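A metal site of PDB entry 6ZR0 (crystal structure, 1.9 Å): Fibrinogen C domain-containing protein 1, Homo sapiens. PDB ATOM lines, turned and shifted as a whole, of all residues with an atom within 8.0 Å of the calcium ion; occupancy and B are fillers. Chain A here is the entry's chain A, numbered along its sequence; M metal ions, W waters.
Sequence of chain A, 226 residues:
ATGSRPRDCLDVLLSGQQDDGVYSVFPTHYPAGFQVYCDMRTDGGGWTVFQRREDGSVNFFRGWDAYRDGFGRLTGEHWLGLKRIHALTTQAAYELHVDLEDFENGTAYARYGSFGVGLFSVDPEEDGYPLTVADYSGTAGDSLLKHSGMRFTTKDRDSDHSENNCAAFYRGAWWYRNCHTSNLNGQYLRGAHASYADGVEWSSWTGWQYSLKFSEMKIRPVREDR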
ATOM      1  N   THR A 153      -7.012  -1.531  13.157  1.00  0.00           N
ATOM      2  CA  THR A 153      -7.247  -2.713  12.283  1.00  0.00           C
ATOM      3  C   THR A 153      -6.550  -2.490  10.928  1.00  0.00           C
ATOM      4  O   THR A 153      -6.738  -1.414  10.336  1.00  0.00           O
ATOM      5  CB  THR A 153      -8.744  -2.982  12.124  1.00  0.00           C
ATOM      6  OG1 THR A 153      -9.221  -3.548  13.346  1.00  0.00           O
ATOM      7  CG2 THR A 153      -9.071  -3.922  10.978  1.00  0.00           C
ATOM      8  N   ARG A 157      -4.710  -7.944  10.186  1.00  0.00           N
ATOM      9  CA  ARG A 157      -4.963  -8.007  11.660  1.00  0.00           C
ATOM     10  C   ARG A 157      -6.275  -7.296  11.987  1.00  0.00           C
ATOM     11  O   ARG A 157      -6.295  -6.052  12.019  1.00  0.00           O
ATOM     12  CB  ARG A 157      -3.783  -7.405  12.442  1.00  0.00           C
ATOM     13  CG  ARG A 157      -3.750  -7.809  13.906  1.00  0.00           C
ATOM     14  CD  ARG A 157      -2.611  -7.126  14.654  1.00  0.00           C
ATOM     15  NE  ARG A 157      -2.411  -7.622  16.011  1.00  0.00           N
ATOM     16  CZ  ARG A 157      -3.077  -7.224  17.084  1.00  0.00           C
ATOM     17  NH1 ARG A 157      -4.032  -6.315  16.987  1.00  0.00           N
ATOM     18  NH2 ARG A 157      -2.801  -7.740  18.271  1.00  0.00           N
ATOM     19  N   ASP A 158      -7.329  -8.082  12.252  1.00  0.00           N
ATOM     20  CA  ASP A 158      -8.739  -7.615  12.414  1.00  0.00           C
ATOM     21  C   ASP A 158      -9.081  -7.532  13.903  1.00  0.00           C
ATOM     22  O   ASP A 158      -9.102  -8.587  14.562  1.00  0.00           O
ATOM     23  CB  ASP A 158      -9.683  -8.550  11.662  1.00  0.00           C
ATOM     24  CG  ASP A 158     -11.143  -8.143  11.717  1.00  0.00           C
ATOM     25  OD1 ASP A 158     -11.503  -7.294  12.559  1.00  0.00           O
ATOM     26  OD2 ASP A 158     -11.924  -8.682  10.904  1.00  0.00           O
ATOM     27  N   SER A 159      -9.373  -6.323  14.404  1.00  0.00           N
ATOM     28  CA  SER A 159      -9.804  -6.043  15.796  1.00  0.00           C
ATOM     29  C   SER A 159     -10.997  -5.080  15.814  1.00  0.00           C
ATOM     30  O   SER A 159     -11.186  -4.390  16.831  1.00  0.00           O
ATOM     31  CB  SER A 159      -8.656  -5.489  16.613  1.00  0.00           C
ATOM     32  OG  SER A 159      -7.495  -6.298  16.488  1.00  0.00           O
ATOM     33  N   ASP A 160     -11.800  -5.066  14.738  1.00  0.00           N
ATOM     34  CA  ASP A 160     -12.957  -4.143  14.564  1.00  0.00           C
ATOM     35  C   ASP A 160     -14.236  -4.849  15.046  1.00  0.00           C
ATOM     36  O   ASP A 160     -14.145  -6.016  15.477  1.00  0.00           O
ATOM     37  CB  ASP A 160     -13.065  -3.635  13.130  1.00  0.00           C
ATOM     38  CG  ASP A 160     -13.307  -4.706  12.082  1.00  0.00           C
ATOM     39  OD1 ASP A 160     -14.087  -5.640  12.364  1.00  0.00           O
ATOM     40  OD2 ASP A 160     -12.715  -4.603  10.987  1.00  0.00           O
ATOM     41  N   HIS A 161     -15.385  -4.156  14.976  1.00  0.00           N
ATOM     42  CA  HIS A 161     -16.716  -4.656  15.399  1.00  0.00           C
ATOM     43  C   HIS A 161     -17.569  -5.051  14.180  1.00  0.00           C
ATOM     44  O   HIS A 161     -18.808  -5.063  14.306  1.00  0.00           O
ATOM     45  CB  HIS A 161     -17.427  -3.612  16.280  1.00  0.00           C
ATOM     46  CG  HIS A 161     -16.837  -3.471  17.642  1.00  0.00           C
ATOM     47  ND1 HIS A 161     -17.291  -2.513  18.537  1.00  0.00           N
ATOM     48  CD2 HIS A 161     -15.830  -4.125  18.255  1.00  0.00           C
ATOM     49  CE1 HIS A 161     -16.601  -2.610  19.655  1.00  0.00           C
ATOM     50  NE2 HIS A 161     -15.686  -3.578  19.507  1.00  0.00           N
ATOM     51  N   SER A 162     -16.922  -5.367  13.056  1.00  0.00           N
ATOM     52  CA  SER A 162     -17.562  -5.898  11.821  1.00  0.00           C
ATOM     53  C   SER A 162     -17.357  -7.415  11.747  1.00  0.00           C
ATOM     54  O   SER A 162     -16.365  -7.906  12.320  1.00  0.00           O
ATOM     55  CB  SER A 162     -17.030  -5.208  10.591  1.00  0.00           C
ATOM     56  OG  SER A 162     -17.566  -5.802   9.416  1.00  0.00           O
ATOM     57  N   GLU A 163     -18.245  -8.126  11.044  1.00  0.00           N
ATOM     58  CA  GLU A 163     -18.139  -9.589  10.788  1.00  0.00           C
ATOM     59  C   GLU A 163     -17.068  -9.838   9.724  1.00  0.00           C
ATOM     60  O   GLU A 163     -16.509 -10.949   9.713  1.00  0.00           O
ATOM     61  CB  GLU A 163     -19.497 -10.157  10.372  1.00  0.00           C
ATOM     62  CG  GLU A 163     -20.514 -10.160  11.504  1.00  0.00           C
ATOM     63  CD  GLU A 163     -21.882 -10.726  11.146  1.00  0.00           C
ATOM     64  OE1 GLU A 163     -22.139 -10.934   9.945  1.00  0.00           O
ATOM     65  OE2 GLU A 163     -22.689 -10.942  12.075  1.00  0.00           O
ATOM     66  N   ASN A 164     -16.781  -8.845   8.870  1.00  0.00           N
ATOM     67  CA  ASN A 164     -15.670  -8.856   7.884  1.00  0.00           C
ATOM     68  C   ASN A 164     -14.544  -7.949   8.392  1.00  0.00           C
ATOM     69  O   ASN A 164     -14.659  -7.443   9.533  1.00  0.00           O
ATOM     70  CB  ASN A 164     -16.160  -8.448   6.487  1.00  0.00           C
ATOM     71  CG  ASN A 164     -16.547  -6.990   6.352  1.00  0.00           C
ATOM     72  OD1 ASN A 164     -16.211  -6.175   7.204  1.00  0.00           O
ATOM     73  ND2 ASN A 164     -17.253  -6.660   5.282  1.00  0.00           N
ATOM     74  N   ASN A 165     -13.491  -7.771   7.583  1.00  0.00           N
ATOM     75  CA  ASN A 165     -12.324  -6.891   7.897  1.00  0.00           C
ATOM     76  C   ASN A 165     -12.565  -5.515   7.242  1.00  0.00           C
ATOM     77  O   ASN A 165     -12.491  -5.442   6.002  1.00  0.00           O
ATOM     78  CB  ASN A 165     -11.017  -7.537   7.441  1.00  0.00           C
ATOM     79  CG  ASN A 165      -9.781  -6.777   7.903  1.00  0.00           C
ATOM     80  OD1 ASN A 165      -9.788  -5.553   7.974  1.00  0.00           O
ATOM     81  ND2 ASN A 165      -8.721  -7.502   8.227  1.00  0.00           N
ATOM     82  N   CYS A 166     -12.828  -4.494   8.054  1.00  0.00           N
ATOM     83  CA  CYS A 166     -13.112  -3.093   7.616  1.00  0.00           C
ATOM     84  C   CYS A 166     -11.940  -2.549   6.801  1.00  0.00           C
ATOM     85  O   CYS A 166     -12.192  -1.857   5.794  1.00  0.00           O
ATOM     86  CB  CYS A 166     -13.359  -2.169   8.802  1.00  0.00           C
ATOM     87  SG  CYS A 166     -14.897  -2.507   9.705  1.00  0.00           S
ATOM     88  N   ALA A 167     -10.696  -2.834   7.214  1.00  0.00           N
ATOM     89  CA  ALA A 167      -9.445  -2.363   6.565  1.00  0.00           C
ATOM     90  C   ALA A 167      -9.351  -2.959   5.155  1.00  0.00           C
ATOM     91  O   ALA A 167      -9.004  -2.200   4.226  1.00  0.00           O
ATOM     92  CB  ALA A 167      -8.247  -2.737   7.399  1.00  0.00           C
ATOM     93  N   TYR A 176     -11.136   1.260  13.233  1.00  0.00           N
ATOM     94  CA  TYR A 176     -12.447   0.903  12.632  1.00  0.00           C
ATOM     95  C   TYR A 176     -13.404   0.393  13.708  1.00  0.00           C
ATOM     96  O   TYR A 176     -12.958  -0.376  14.589  1.00  0.00           O
ATOM     97  CB  TYR A 176     -12.281  -0.158  11.548  1.00  0.00           C
ATOM     98  CG  TYR A 176     -11.626   0.315  10.269  1.00  0.00           C
ATOM     99  CD1 TYR A 176     -12.251   1.223   9.437  1.00  0.00           C
ATOM    100  CD2 TYR A 176     -10.394  -0.177   9.884  1.00  0.00           C
ATOM    101  CE1 TYR A 176     -11.662   1.646   8.255  1.00  0.00           C
ATOM    102  CE2 TYR A 176      -9.784   0.241   8.716  1.00  0.00           C
ATOM    103  CZ  TYR A 176     -10.415   1.159   7.889  1.00  0.00           C
ATOM    104  OH  TYR A 176      -9.810   1.567   6.737  1.00  0.00           O
ATOM    105  N   ARG A 177     -14.671   0.794  13.630  1.00  0.00           N
ATOM    106  CA  ARG A 177     -15.798   0.227  14.430  1.00  0.00           C
ATOM    107  C   ARG A 177     -16.602  -0.708  13.512  1.00  0.00           C
ATOM    108  O   ARG A 177     -16.281  -1.914  13.493  1.00  0.00           O
ATOM    109  CB  ARG A 177     -16.631   1.348  15.054  1.00  0.00           C
ATOM    110  CG  ARG A 177     -17.777   0.861  15.920  1.00  0.00           C
ATOM    111  CD  ARG A 177     -18.603   1.998  16.496  1.00  0.00           C
ATOM    112  NE  ARG A 177     -17.842   2.835  17.417  1.00  0.00           N
ATOM    113  CZ  ARG A 177     -17.579   2.535  18.691  1.00  0.00           C
ATOM    114  NH1 ARG A 177     -17.997   1.400  19.218  1.00  0.00           N
ATOM    115  NH2 ARG A 177     -16.880   3.385  19.428  1.00  0.00           N
ATOM    116  N   ASN A 178     -17.568  -0.180  12.754  1.00  0.00           N
ATOM    117  CA  ASN A 178     -18.472  -0.972  11.881  1.00  0.00           C
ATOM    118  C   ASN A 178     -19.125  -0.050  10.838  1.00  0.00           C
ATOM    119  O   ASN A 178     -20.350   0.049  10.795  1.00  0.00           O
ATOM    120  CB  ASN A 178     -19.522  -1.712  12.731  1.00  0.00           C
ATOM    121  CG  ASN A 178     -20.288  -2.763  11.955  1.00  0.00           C
ATOM    122  OD1 ASN A 178     -19.747  -3.426  11.065  1.00  0.00           O
ATOM    123  ND2 ASN A 178     -21.558  -2.925  12.282  1.00  0.00           N
ATOM    124  N   CYS A 179     -18.311   0.602   9.986  1.00  0.00           N
ATOM    125  CA  CYS A 179     -16.864   0.489   9.981  1.00  0.00           C
ATOM    126  C   CYS A 179     -16.222   1.838  10.331  1.00  0.00           C
ATOM    127  O   CYS A 179     -15.365   1.852  11.236  1.00  0.00           O
ATOM    128  CB  CYS A 179     -16.348  -0.021   8.641  1.00  0.00           C
ATOM    129  SG  CYS A 179     -16.390  -1.823   8.482  1.00  0.00           S
HETATM  130 CA    CA M   1     -14.030  -7.930  11.911  1.00  0.00          CA
HETATM  131  O   HOH W   1     -13.999 -10.318  12.104  1.00  0.00           O
HETATM  132  O   HOH W   2     -14.227  -8.456  14.300  1.00  0.00           O
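Within 4 Å of the calcium ion: Asp 158, Asp 160, Ser 162 and Asn 164.
The calcium ion is bound by OD1 of Asp 160 (2.3 Å), O of Ser 162 (2.4 Å), water W1 (2.4 Å), OD2 of Asp 158 (2.5 Å), water W2 (2.5 Å), O of Asn 164 (2.5 Å) and OD1 of Asp 158 (2.7 Å).
The calcium ion has seven donor atoms within binding distance.
The backbone NH of Cys 166 lies within hydrogen-bond range of the side-chain carboxylate of Asp 160.
The backbone NH (N) of Asp 160 is in hydrogen-bond range of the side-chain hydroxyl (OG1) of Thr 153 (3.3 Å).
The side-chain hydroxyl of Ser 162 lies within hydrogen-bond range of the side-chain amide oxygen of Asn 164 (2.6 Å).
The side-chain sulfur (SG) of Cys 166 is disulfide-bonded to the side-chain sulfur (SG) of Cys 179 (2.0 Å).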
